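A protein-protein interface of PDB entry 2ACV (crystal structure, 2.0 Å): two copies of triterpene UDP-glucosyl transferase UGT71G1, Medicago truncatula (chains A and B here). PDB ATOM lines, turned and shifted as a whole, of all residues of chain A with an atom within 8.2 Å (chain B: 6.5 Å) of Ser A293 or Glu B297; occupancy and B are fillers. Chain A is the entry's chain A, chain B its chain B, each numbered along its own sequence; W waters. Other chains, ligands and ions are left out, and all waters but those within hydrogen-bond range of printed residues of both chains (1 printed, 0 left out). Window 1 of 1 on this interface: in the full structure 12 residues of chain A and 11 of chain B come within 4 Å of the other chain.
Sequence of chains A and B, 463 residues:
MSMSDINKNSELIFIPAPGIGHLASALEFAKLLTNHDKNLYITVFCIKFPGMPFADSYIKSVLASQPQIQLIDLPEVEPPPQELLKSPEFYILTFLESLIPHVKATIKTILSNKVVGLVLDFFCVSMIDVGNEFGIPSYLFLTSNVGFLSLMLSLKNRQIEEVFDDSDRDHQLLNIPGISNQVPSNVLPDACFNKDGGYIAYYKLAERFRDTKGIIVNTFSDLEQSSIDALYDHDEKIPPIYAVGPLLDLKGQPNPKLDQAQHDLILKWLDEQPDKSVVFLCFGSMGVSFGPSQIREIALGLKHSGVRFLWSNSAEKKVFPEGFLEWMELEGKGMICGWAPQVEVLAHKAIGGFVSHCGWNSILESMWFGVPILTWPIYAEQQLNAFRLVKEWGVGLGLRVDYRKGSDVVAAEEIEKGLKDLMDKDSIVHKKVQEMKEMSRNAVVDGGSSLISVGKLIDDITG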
ATOM      1  N   PHE A 290      31.819  16.817  -4.270  1.00  0.00           N
ATOM      2  CA  PHE A 290      30.686  17.438  -4.931  1.00  0.00           C
ATOM      3  C   PHE A 290      29.469  16.608  -4.536  1.00  0.00           C
ATOM      4  O   PHE A 290      29.621  15.500  -4.032  1.00  0.00           O
ATOM      5  CB  PHE A 290      30.885  17.363  -6.445  1.00  0.00           C
ATOM      6  CG  PHE A 290      31.976  18.255  -6.961  1.00  0.00           C
ATOM      7  CD1 PHE A 290      31.854  19.640  -6.876  1.00  0.00           C
ATOM      8  CD2 PHE A 290      33.104  17.717  -7.574  1.00  0.00           C
ATOM      9  CE1 PHE A 290      32.835  20.481  -7.395  1.00  0.00           C
ATOM     10  CE2 PHE A 290      34.096  18.553  -8.099  1.00  0.00           C
ATOM     11  CZ  PHE A 290      33.959  19.936  -8.008  1.00  0.00           C
ATOM     12  N   GLY A 291      28.272  17.144  -4.755  1.00  0.00           N
ATOM     13  CA  GLY A 291      27.063  16.405  -4.433  1.00  0.00           C
ATOM     14  C   GLY A 291      26.881  15.247  -5.403  1.00  0.00           C
ATOM     15  O   GLY A 291      27.584  15.182  -6.417  1.00  0.00           O
ATOM     16  N   PRO A 292      25.933  14.329  -5.141  1.00  0.00           N
ATOM     17  CA  PRO A 292      25.675  13.166  -5.997  1.00  0.00           C
ATOM     18  C   PRO A 292      25.469  13.463  -7.484  1.00  0.00           C
ATOM     19  O   PRO A 292      26.107  12.840  -8.341  1.00  0.00           O
ATOM     20  CB  PRO A 292      24.439  12.535  -5.354  1.00  0.00           C
ATOM     21  CG  PRO A 292      24.612  12.876  -3.911  1.00  0.00           C
ATOM     22  CD  PRO A 292      25.008  14.334  -3.992  1.00  0.00           C
ATOM     23  N   SER A 293      24.575  14.401  -7.787  1.00  0.00           N
ATOM     24  CA  SER A 293      24.293  14.771  -9.179  1.00  0.00           C
ATOM     25  C   SER A 293      25.554  15.213  -9.904  1.00  0.00           C
ATOM     26  O   SER A 293      25.814  14.786 -11.027  1.00  0.00           O
ATOM     27  CB  SER A 293      23.274  15.912  -9.234  1.00  0.00           C
ATOM     28  OG  SER A 293      22.072  15.538  -8.591  1.00  0.00           O
ATOM     29  N   GLN A 294      26.335  16.079  -9.267  1.00  0.00           N
ATOM     30  CA  GLN A 294      27.562  16.577  -9.881  1.00  0.00           C
ATOM     31  C   GLN A 294      28.581  15.458 -10.112  1.00  0.00           C
ATOM     32  O   GLN A 294      29.282  15.443 -11.123  1.00  0.00           O
ATOM     33  CB  GLN A 294      28.184  17.669  -9.014  1.00  0.00           C
ATOM     34  CG  GLN A 294      29.451  18.254  -9.626  1.00  0.00           C
ATOM     35  CD  GLN A 294      29.173  18.961 -10.935  1.00  0.00           C
ATOM     36  OE1 GLN A 294      28.812  20.147 -10.951  1.00  0.00           O
ATOM     37  NE2 GLN A 294      29.318  18.233 -12.045  1.00  0.00           N
ATOM     38  N   ILE A 295      28.671  14.531  -9.167  1.00  0.00           N
ATOM     39  CA  ILE A 295      29.592  13.411  -9.304  1.00  0.00           C
ATOM     40  C   ILE A 295      29.180  12.589 -10.531  1.00  0.00           C
ATOM     41  O   ILE A 295      30.030  12.174 -11.319  1.00  0.00           O
ATOM     42  CB  ILE A 295      29.568  12.495  -8.046  1.00  0.00           C
ATOM     43  CG1 ILE A 295      30.095  13.260  -6.818  1.00  0.00           C
ATOM     44  CG2 ILE A 295      30.395  11.229  -8.303  1.00  0.00           C
ATOM     45  CD1 ILE A 295      31.573  13.645  -6.886  1.00  0.00           C
ATOM     46  N   ARG A 296      27.876  12.357 -10.693  1.00  0.00           N
ATOM     47  CA  ARG A 296      27.367  11.581 -11.837  1.00  0.00           C
ATOM     48  C   ARG A 296      27.709  12.244 -13.162  1.00  0.00           C
ATOM     49  O   ARG A 296      28.069  11.565 -14.128  1.00  0.00           O
ATOM     50  CB  ARG A 296      25.841  11.416 -11.763  1.00  0.00           C
ATOM     51  CG  ARG A 296      25.364  10.461 -10.715  1.00  0.00           C
ATOM     52  CD  ARG A 296      23.849  10.588 -10.494  1.00  0.00           C
ATOM     53  NE  ARG A 296      23.545   9.944  -9.235  1.00  0.00           N
ATOM     54  CZ  ARG A 296      22.852  10.480  -8.245  1.00  0.00           C
ATOM     55  NH1 ARG A 296      22.337  11.709  -8.332  1.00  0.00           N
ATOM     56  NH2 ARG A 296      22.716   9.774  -7.142  1.00  0.00           N
ATOM     57  N   GLU A 297      27.584  13.569 -13.207  1.00  0.00           N
ATOM     58  CA  GLU A 297      27.874  14.314 -14.425  1.00  0.00           C
ATOM     59  C   GLU A 297      29.360  14.270 -14.772  1.00  0.00           C
ATOM     60  O   GLU A 297      29.726  14.225 -15.945  1.00  0.00           O
ATOM     61  CB  GLU A 297      27.384  15.762 -14.296  1.00  0.00           C
ATOM     62  CG  GLU A 297      25.851  15.897 -14.282  1.00  0.00           C
ATOM     63  CD  GLU A 297      25.189  15.394 -15.566  1.00  0.00           C
ATOM     64  OE1 GLU A 297      25.586  15.850 -16.657  1.00  0.00           O
ATOM     65  OE2 GLU A 297      24.271  14.548 -15.488  1.00  0.00           O
ATOM     66  N   ILE A 298      30.217  14.280 -13.756  1.00  0.00           N
ATOM     67  CA  ILE A 298      31.652  14.196 -13.988  1.00  0.00           C
ATOM     68  C   ILE A 298      31.970  12.802 -14.537  1.00  0.00           C
ATOM     69  O   ILE A 298      32.709  12.659 -15.507  1.00  0.00           O
ATOM     70  CB  ILE A 298      32.451  14.426 -12.674  1.00  0.00           C
ATOM     71  CG1 ILE A 298      32.258  15.870 -12.194  1.00  0.00           C
ATOM     72  CG2 ILE A 298      33.939  14.107 -12.903  1.00  0.00           C
ATOM     73  CD1 ILE A 298      32.836  16.162 -10.810  1.00  0.00           C
ATOM     74  N   ALA A 299      31.410  11.776 -13.904  1.00  0.00           N
ATOM     75  CA  ALA A 299      31.626  10.395 -14.327  1.00  0.00           C
ATOM     76  C   ALA A 299      31.223  10.184 -15.789  1.00  0.00           C
ATOM     77  O   ALA A 299      31.979   9.606 -16.576  1.00  0.00           O
ATOM     78  CB  ALA A 299      30.832   9.445 -13.431  1.00  0.00           C
ATOM     79  N   LEU A 300      30.027  10.643 -16.146  1.00  0.00           N
ATOM     80  CA  LEU A 300      29.542  10.501 -17.516  1.00  0.00           C
ATOM     81  C   LEU A 300      30.406  11.287 -18.508  1.00  0.00           C
ATOM     82  O   LEU A 300      30.721  10.790 -19.591  1.00  0.00           O
ATOM     83  CB  LEU A 300      28.090  10.970 -17.613  1.00  0.00           C
ATOM     84  CG  LEU A 300      27.429  10.805 -18.987  1.00  0.00           C
ATOM     85  CD1 LEU A 300      27.327   9.321 -19.324  1.00  0.00           C
ATOM     86  CD2 LEU A 300      26.036  11.443 -18.979  1.00  0.00           C
ATOM     87  N   VAL A 319      26.432   6.374  -5.259  1.00  0.00           N
ATOM     88  CA  VAL A 319      26.145   7.599  -6.001  1.00  0.00           C
ATOM     89  C   VAL A 319      26.433   7.554  -7.511  1.00  0.00           C
ATOM     90  O   VAL A 319      25.762   8.225  -8.298  1.00  0.00           O
ATOM     91  CB  VAL A 319      26.940   8.789  -5.392  1.00  0.00           C
ATOM     92  CG1 VAL A 319      26.760  10.030  -6.238  1.00  0.00           C
ATOM     93  CG2 VAL A 319      26.460   9.058  -3.972  1.00  0.00           C
ATOM     94  N   PHE A 320      27.418   6.762  -7.911  1.00  0.00           N
ATOM     95  CA  PHE A 320      27.822   6.688  -9.315  1.00  0.00           C
ATOM     96  C   PHE A 320      26.776   6.171 -10.302  1.00  0.00           C
ATOM     97  O   PHE A 320      25.887   5.411  -9.939  1.00  0.00           O
ATOM     98  CB  PHE A 320      29.116   5.864  -9.418  1.00  0.00           C
ATOM     99  CG  PHE A 320      30.307   6.542  -8.796  1.00  0.00           C
ATOM    100  CD1 PHE A 320      31.113   7.394  -9.552  1.00  0.00           C
ATOM    101  CD2 PHE A 320      30.584   6.382  -7.442  1.00  0.00           C
ATOM    102  CE1 PHE A 320      32.179   8.084  -8.970  1.00  0.00           C
ATOM    103  CE2 PHE A 320      31.648   7.063  -6.843  1.00  0.00           C
ATOM    104  CZ  PHE A 320      32.448   7.920  -7.608  1.00  0.00           C
ATOM    105  N   PRO A 321      26.864   6.598 -11.575  1.00  0.00           N
ATOM    106  CA  PRO A 321      25.888   6.130 -12.564  1.00  0.00           C
ATOM    107  C   PRO A 321      25.942   4.612 -12.613  1.00  0.00           C
ATOM    108  O   PRO A 321      27.024   4.032 -12.518  1.00  0.00           O
ATOM    109  CB  PRO A 321      26.386   6.754 -13.875  1.00  0.00           C
ATOM    110  CG  PRO A 321      27.087   8.000 -13.414  1.00  0.00           C
ATOM    111  CD  PRO A 321      27.843   7.507 -12.194  1.00  0.00           C
ATOM    112  N   VAL A 409      24.935  22.588 -11.052  1.00  0.00           N
ATOM    113  CA  VAL A 409      25.734  21.451 -11.484  1.00  0.00           C
ATOM    114  C   VAL A 409      26.328  21.733 -12.869  1.00  0.00           C
ATOM    115  O   VAL A 409      25.683  22.338 -13.727  1.00  0.00           O
ATOM    116  CB  VAL A 409      24.891  20.149 -11.565  1.00  0.00           C
ATOM    117  CG1 VAL A 409      24.196  19.886 -10.237  1.00  0.00           C
ATOM    118  CG2 VAL A 409      23.880  20.257 -12.676  1.00  0.00           C
ATOM    119  N   VAL A 410      27.571  21.313 -13.068  1.00  0.00           N
ATOM    120  CA  VAL A 410      28.249  21.471 -14.346  1.00  0.00           C
ATOM    121  C   VAL A 410      27.922  20.181 -15.091  1.00  0.00           C
ATOM    122  O   VAL A 410      28.241  19.098 -14.611  1.00  0.00           O
ATOM    123  CB  VAL A 410      29.770  21.596 -14.144  1.00  0.00           C
ATOM    124  CG1 VAL A 410      30.485  21.672 -15.496  1.00  0.00           C
ATOM    125  CG2 VAL A 410      30.068  22.828 -13.310  1.00  0.00           C
ATOM    126  N   ALA A 411      27.269  20.307 -16.247  1.00  0.00           N
ATOM    127  CA  ALA A 411      26.852  19.160 -17.051  1.00  0.00           C
ATOM    128  C   ALA A 411      27.977  18.369 -17.717  1.00  0.00           C
ATOM    129  O   ALA A 411      29.035  18.910 -18.032  1.00  0.00           O
ATOM    130  CB  ALA A 411      25.855  19.625 -18.111  1.00  0.00           C
ATOM    131  N   ALA A 412      27.723  17.081 -17.946  1.00  0.00           N
ATOM    132  CA  ALA A 412      28.701  16.192 -18.578  1.00  0.00           C
ATOM    133  C   ALA A 412      29.157  16.716 -19.941  1.00  0.00           C
ATOM    134  O   ALA A 412      30.338  16.628 -20.292  1.00  0.00           O
ATOM    135  CB  ALA A 412      28.103  14.786 -18.738  1.00  0.00           C
ATOM    136  N   ILE A 415      31.699  19.352 -19.505  1.00  0.00           N
ATOM    137  CA  ILE A 415      32.910  18.754 -18.953  1.00  0.00           C
ATOM    138  C   ILE A 415      33.673  18.026 -20.064  1.00  0.00           C
ATOM    139  O   ILE A 415      34.890  18.152 -20.183  1.00  0.00           O
ATOM    140  CB  ILE A 415      32.556  17.765 -17.806  1.00  0.00           C
ATOM    141  CG1 ILE A 415      31.977  18.554 -16.625  1.00  0.00           C
ATOM    142  CG2 ILE A 415      33.793  16.983 -17.378  1.00  0.00           C
ATOM    143  CD1 ILE A 415      31.411  17.713 -15.510  1.00  0.00           C
ATOM    144  N   PRO B 292      19.794  18.198 -20.370  1.00  0.00           N
ATOM    145  CA  PRO B 292      20.378  16.851 -20.293  1.00  0.00           C
ATOM    146  C   PRO B 292      20.625  16.337 -18.865  1.00  0.00           C
ATOM    147  O   PRO B 292      20.199  15.237 -18.521  1.00  0.00           O
ATOM    148  CB  PRO B 292      21.676  16.991 -21.087  1.00  0.00           C
ATOM    149  CG  PRO B 292      21.316  18.026 -22.130  1.00  0.00           C
ATOM    150  CD  PRO B 292      20.560  19.049 -21.305  1.00  0.00           C
ATOM    151  N   SER B 293      21.306  17.130 -18.041  1.00  0.00           N
ATOM    152  CA  SER B 293      21.591  16.740 -16.661  1.00  0.00           C
ATOM    153  C   SER B 293      20.310  16.387 -15.910  1.00  0.00           C
ATOM    154  O   SER B 293      20.220  15.335 -15.284  1.00  0.00           O
ATOM    155  CB  SER B 293      22.299  17.874 -15.911  1.00  0.00           C
ATOM    156  OG  SER B 293      23.528  18.211 -16.531  1.00  0.00           O
ATOM    157  N   GLN B 294      19.323  17.277 -15.976  1.00  0.00           N
ATOM    158  CA  GLN B 294      18.053  17.063 -15.293  1.00  0.00           C
ATOM    159  C   GLN B 294      17.316  15.827 -15.813  1.00  0.00           C
ATOM    160  O   GLN B 294      16.692  15.096 -15.032  1.00  0.00           O
ATOM    161  CB  GLN B 294      17.163  18.302 -15.427  1.00  0.00           C
ATOM    162  CG  GLN B 294      15.858  18.177 -14.646  1.00  0.00           C
ATOM    163  CD  GLN B 294      16.103  18.092 -13.149  1.00  0.00           C
ATOM    164  OE1 GLN B 294      16.222  19.112 -12.470  1.00  0.00           O
ATOM    165  NE2 GLN B 294      16.203  16.872 -12.631  1.00  0.00           N
ATOM    166  N   ILE B 295      17.379  15.591 -17.123  1.00  0.00           N
ATOM    167  CA  ILE B 295      16.726  14.415 -17.704  1.00  0.00           C
ATOM    168  C   ILE B 295      17.368  13.145 -17.124  1.00  0.00           C
ATOM    169  O   ILE B 295      16.677  12.182 -16.816  1.00  0.00           O
ATOM    170  CB  ILE B 295      16.862  14.375 -19.260  1.00  0.00           C
ATOM    171  CG1 ILE B 295      15.979  15.452 -19.905  1.00  0.00           C
ATOM    172  CG2 ILE B 295      16.475  12.994 -19.786  1.00  0.00           C
ATOM    173  CD1 ILE B 295      14.473  15.214 -19.734  1.00  0.00           C
ATOM    174  N   ARG B 296      18.692  13.148 -16.984  1.00  0.00           N
ATOM    175  CA  ARG B 296      19.401  11.996 -16.431  1.00  0.00           C
ATOM    176  C   ARG B 296      19.010  11.730 -14.975  1.00  0.00           C
ATOM    177  O   ARG B 296      18.883  10.582 -14.556  1.00  0.00           O
ATOM    178  CB  ARG B 296      20.915  12.213 -16.502  1.00  0.00           C
ATOM    179  CG  ARG B 296      21.497  12.005 -17.878  1.00  0.00           C
ATOM    180  CD  ARG B 296      22.886  12.630 -17.983  1.00  0.00           C
ATOM    181  NE  ARG B 296      23.085  12.962 -19.374  1.00  0.00           N
ATOM    182  CZ  ARG B 296      23.639  14.069 -19.824  1.00  0.00           C
ATOM    183  NH1 ARG B 296      24.086  15.011 -18.994  1.00  0.00           N
ATOM    184  NH2 ARG B 296      23.718  14.228 -21.129  1.00  0.00           N
ATOM    185  N   GLU B 297      18.836  12.800 -14.204  1.00  0.00           N
ATOM    186  CA  GLU B 297      18.464  12.663 -12.797  1.00  0.00           C
ATOM    187  C   GLU B 297      17.028  12.131 -12.658  1.00  0.00           C
ATOM    188  O   GLU B 297      16.738  11.363 -11.740  1.00  0.00           O
ATOM    189  CB  GLU B 297      18.631  14.004 -12.080  1.00  0.00           C
ATOM    190  CG  GLU B 297      20.085  14.469 -11.947  1.00  0.00           C
ATOM    191  CD  GLU B 297      20.929  13.546 -11.053  1.00  0.00           C
ATOM    192  OE1 GLU B 297      20.475  13.228  -9.937  1.00  0.00           O
ATOM    193  OE2 GLU B 297      22.049  13.145 -11.459  1.00  0.00           O
ATOM    194  N   ILE B 298      16.136  12.527 -13.566  1.00  0.00           N
ATOM    195  CA  ILE B 298      14.756  12.034 -13.535  1.00  0.00           C
ATOM    196  C   ILE B 298      14.772  10.537 -13.876  1.00  0.00           C
ATOM    197  O   ILE B 298      14.083   9.735 -13.245  1.00  0.00           O
ATOM    198  CB  ILE B 298      13.856  12.774 -14.563  1.00  0.00           C
ATOM    199  CG1 ILE B 298      13.643  14.231 -14.133  1.00  0.00           C
ATOM    200  CG2 ILE B 298      12.499  12.078 -14.677  1.00  0.00           C
ATOM    201  CD1 ILE B 298      12.905  15.065 -15.175  1.00  0.00           C
ATOM    202  N   ALA B 299      15.572  10.166 -14.870  1.00  0.00           N
ATOM    203  CA  ALA B 299      15.677   8.766 -15.287  1.00  0.00           C
ATOM    204  C   ALA B 299      16.188   7.868 -14.152  1.00  0.00           C
ATOM    205  O   ALA B 299      15.634   6.798 -13.886  1.00  0.00           O
ATOM    206  CB  ALA B 299      16.603   8.655 -16.495  1.00  0.00           C
ATOM    207  N   LEU B 300      17.256   8.298 -13.493  1.00  0.00           N
ATOM    208  CA  LEU B 300      17.807   7.516 -12.398  1.00  0.00           C
ATOM    209  C   LEU B 300      16.790   7.453 -11.266  1.00  0.00           C
ATOM    210  O   LEU B 300      16.538   6.380 -10.711  1.00  0.00           O
ATOM    211  CB  LEU B 300      19.123   8.133 -11.910  1.00  0.00           C
ATOM    212  CG  LEU B 300      19.851   7.415 -10.768  1.00  0.00           C
ATOM    213  CD1 LEU B 300      20.135   5.953 -11.134  1.00  0.00           C
ATOM    214  CD2 LEU B 300      21.154   8.153 -10.476  1.00  0.00           C
ATOM    215  N   GLY B 301      16.201   8.601 -10.934  1.00  0.00           N
ATOM    216  CA  GLY B 301      15.203   8.646  -9.879  1.00  0.00           C
ATOM    217  C   GLY B 301      14.071   7.659 -10.129  1.00  0.00           C
ATOM    218  O   GLY B 301      13.669   6.917  -9.229  1.00  0.00           O
ATOM    219  N   LEU B 302      13.548   7.651 -11.352  1.00  0.00           N
ATOM    220  CA  LEU B 302      12.469   6.740 -11.709  1.00  0.00           C
ATOM    221  C   LEU B 302      12.900   5.281 -11.566  1.00  0.00           C
ATOM    222  O   LEU B 302      12.214   4.489 -10.924  1.00  0.00           O
ATOM    223  CB  LEU B 302      11.998   7.001 -13.147  1.00  0.00           C
ATOM    224  CG  LEU B 302      11.166   8.269 -13.359  1.00  0.00           C
ATOM    225  CD1 LEU B 302      11.062   8.589 -14.847  1.00  0.00           C
ATOM    226  CD2 LEU B 302       9.784   8.072 -12.747  1.00  0.00           C
ATOM    227  N   TRP B 311       6.640   8.211 -19.263  1.00  0.00           N
ATOM    228  CA  TRP B 311       7.261   9.526 -19.247  1.00  0.00           C
ATOM    229  C   TRP B 311       7.260  10.236 -20.602  1.00  0.00           C
ATOM    230  O   TRP B 311       7.946   9.824 -21.533  1.00  0.00           O
ATOM    231  CB  TRP B 311       8.682   9.337 -18.709  1.00  0.00           C
ATOM    232  CG  TRP B 311       9.575  10.525 -18.651  1.00  0.00           C
ATOM    233  CD1 TRP B 311       9.224  11.845 -18.746  1.00  0.00           C
ATOM    234  CD2 TRP B 311      10.986  10.498 -18.419  1.00  0.00           C
ATOM    235  NE1 TRP B 311      10.337  12.640 -18.583  1.00  0.00           N
ATOM    236  CE2 TRP B 311      11.430  11.838 -18.381  1.00  0.00           C
ATOM    237  CE3 TRP B 311      11.919   9.466 -18.236  1.00  0.00           C
ATOM    238  CZ2 TRP B 311      12.767  12.176 -18.168  1.00  0.00           C
ATOM    239  CZ3 TRP B 311      13.254   9.801 -18.022  1.00  0.00           C
ATOM    240  CH2 TRP B 311      13.665  11.147 -17.990  1.00  0.00           C
ATOM    241  N   PRO B 321      20.760   8.132 -19.270  1.00  0.00           N
ATOM    242  CA  PRO B 321      21.854   7.393 -18.637  1.00  0.00           C
ATOM    243  C   PRO B 321      22.117   6.116 -19.416  1.00  0.00           C
ATOM    244  O   PRO B 321      21.189   5.509 -19.952  1.00  0.00           O
ATOM    245  CB  PRO B 321      21.308   7.100 -17.242  1.00  0.00           C
ATOM    246  CG  PRO B 321      20.389   8.250 -16.991  1.00  0.00           C
ATOM    247  CD  PRO B 321      19.677   8.390 -18.305  1.00  0.00           C
ATOM    248  N   VAL B 409      19.476  21.764 -10.892  1.00  0.00           N
ATOM    249  CA  VAL B 409      18.925  20.429 -11.075  1.00  0.00           C
ATOM    250  C   VAL B 409      18.363  19.805  -9.801  1.00  0.00           C
ATOM    251  O   VAL B 409      18.931  19.949  -8.723  1.00  0.00           O
ATOM    252  CB  VAL B 409      19.988  19.468 -11.651  1.00  0.00           C
ATOM    253  CG1 VAL B 409      20.645  20.090 -12.877  1.00  0.00           C
ATOM    254  CG2 VAL B 409      21.021  19.153 -10.596  1.00  0.00           C
ATOM    255  N   VAL B 410      17.226  19.128  -9.943  1.00  0.00           N
ATOM    256  CA  VAL B 410      16.587  18.422  -8.836  1.00  0.00           C
ATOM    257  C   VAL B 410      17.187  17.010  -8.940  1.00  0.00           C
ATOM    258  O   VAL B 410      17.003  16.327  -9.948  1.00  0.00           O
ATOM    259  CB  VAL B 410      15.050  18.359  -9.025  1.00  0.00           C
ATOM    260  CG1 VAL B 410      14.417  17.590  -7.883  1.00  0.00           C
ATOM    261  CG2 VAL B 410      14.466  19.780  -9.097  1.00  0.00           C
ATOM    262  N   ALA B 411      17.913  16.592  -7.907  1.00  0.00           N
ATOM    263  CA  ALA B 411      18.591  15.298  -7.895  1.00  0.00           C
ATOM    264  C   ALA B 411      17.712  14.055  -7.851  1.00  0.00           C
ATOM    265  O   ALA B 411      16.593  14.084  -7.338  1.00  0.00           O
ATOM    266  CB  ALA B 411      19.600  15.258  -6.735  1.00  0.00           C
ATOM    267  N   ALA B 412      18.254  12.951  -8.373  1.00  0.00           N
ATOM    268  CA  ALA B 412      17.543  11.672  -8.405  1.00  0.00           C
ATOM    269  C   ALA B 412      17.033  11.260  -7.029  1.00  0.00           C
ATOM    270  O   ALA B 412      15.920  10.746  -6.898  1.00  0.00           O
ATOM    271  CB  ALA B 412      18.460  10.575  -8.954  1.00  0.00           C
ATOM    272  N   GLU B 413      17.854  11.470  -6.007  1.00  0.00           N
ATOM    273  CA  GLU B 413      17.462  11.100  -4.650  1.00  0.00           C
ATOM    274  C   GLU B 413      16.174  11.799  -4.228  1.00  0.00           C
ATOM    275  O   GLU B 413      15.275  11.172  -3.667  1.00  0.00           O
ATOM    276  CB  GLU B 413      18.576  11.432  -3.649  1.00  0.00           C
ATOM    277  CG  GLU B 413      19.803  10.531  -3.710  1.00  0.00           C
ATOM    278  CD  GLU B 413      20.726  10.827  -4.888  1.00  0.00           C
ATOM    279  OE1 GLU B 413      20.699  11.951  -5.432  1.00  0.00           O
ATOM    280  OE2 GLU B 413      21.503   9.929  -5.255  1.00  0.00           O
ATOM    281  N   ILE B 415      13.874  13.123  -6.228  1.00  0.00           N
ATOM    282  CA  ILE B 415      12.804  12.662  -7.105  1.00  0.00           C
ATOM    283  C   ILE B 415      12.292  11.294  -6.658  1.00  0.00           C
ATOM    284  O   ILE B 415      11.085  11.069  -6.590  1.00  0.00           O
ATOM    285  CB  ILE B 415      13.302  12.605  -8.566  1.00  0.00           C
ATOM    286  CG1 ILE B 415      13.664  14.025  -9.017  1.00  0.00           C
ATOM    287  CG2 ILE B 415      12.244  11.974  -9.468  1.00  0.00           C
ATOM    288  CD1 ILE B 415      14.326  14.111 -10.380  1.00  0.00           C
HETATM  289  O   HOH W   1      23.233  12.600 -13.740  1.00  0.00           O
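Of the 19 printed residues of chain A, 7 touch a printed residue of chain B. Printed residues of chain A that touch a printed residue of chain B: Pro A292, Ser A293, Arg A296, Glu A297, Leu A300, Val A409 and Ala A411. Hydrophobic or aromatic side chains of chain A within 4 Å of the printed part of chain B: Pro A292, Leu A300, Val A409 and Ala A411. Along chain A the printed residues that touch a printed residue of chain B span positions 292 to 411. Among the printed residues, Asp or Glu carboxylates within 4 Å of a Lys or Arg side-chain nitrogen of the other chain: Arg A296 with Glu B297, Arg A296 with Glu B413 and Glu A297 with Arg B296.
Of chain B, only Glu B297 and Ala B411 come within 4 Å of Ser A293. Printed residues of chain A within 4 Å of Glu B297: Ser A293 and Arg A296. Of the printed residues of chain B, Arg A296 touches Glu B297, Leu B300 and Glu B413. Of the printed residues of chain B, Pro A292 touches Glu B413 (3.8 Å). Of the printed residues of chain B, Ala A411 touches Ser B293 (3.1 Å). Of the printed residues of chain A, Arg B296 touches Glu A297 and Leu A300. Ala B299 touches none of the printed residues of chain A. Phe A290 touches none of the printed residues of chain B. The nearest residue of chain B that does not touch Ser A293 is Val B409 (4.2 Å). The nearest residue of chain A that does not touch Glu B297 is Glu A297 (4.8 Å).
The backbone carbonyl oxygen (O) of Val A319 lies within hydrogen-bond range of the guanidinium group (NE) of Arg A296 (3.0 Å). The side-chain carboxylate of Glu A297 lies within hydrogen-bond range of the backbone NH of Ala A412, at 2.8 Å. OE1 of Glu B297 lies within hydrogen-bond range of N of Ala B412, 2.7 Å away.
Ser A293 touches Glu B297, and with the chains exchanged Glu A297 touches Ser B293. Ser A293 touches Ala B411, and with the chains exchanged Ala A411 touches Ser B293. Arg A296 touches Leu B300, and with the chains exchanged Leu A300 touches Arg B296. Val A409 touches its own counterpart, Val B409. Positions printed for both chains: 292, 293, 294, 295, 296, 297, 298, 299, 300, 321, 409, 410, 411, 412 and 415. Of the 11 pairs that touch across the chains among the printed residues, 9 have their exchanged pair printed and touching as well.
CB of Pro A292 touches OE1 of Glu B413, 3.8 Å away. Ser A293 touches Ala B411. NE of Arg A296 touches CD2 of Leu B300 (3.2 Å). NE of Arg B296 touches CD2 of Leu A300 (3.3 Å). CG1 of Val B409 touches CG2 of Val A409, 3.2 Å away. Ala A411 touches Ser B293 (CB to OG, 3.1 Å).
Water W1 lies within hydrogen-bond range of OE2 of Glu B297 (2.6 Å) and OE2 of Glu A297 (2.8 Å).
OE1 of Glu B297 is in hydrogen-bond range of OG of Ser A293 (3.1 Å). The side-chain carboxylate of Glu B297 is in salt-bridge range of the guanidinium group of Arg A296 (2.9 Å). The guanidinium group (NH1) of Arg A296 is in salt-bridge range of the side-chain carboxylate (OE1) of Glu B413, 3.3 Å away. The side-chain hydroxyl of Ser B293 is in hydrogen-bond range of the side-chain carboxylate of Glu A297 (3.1 Å). NH1 of Arg B296 lies within salt-bridge range of OE1 of Glu A297, 2.9 Å away.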
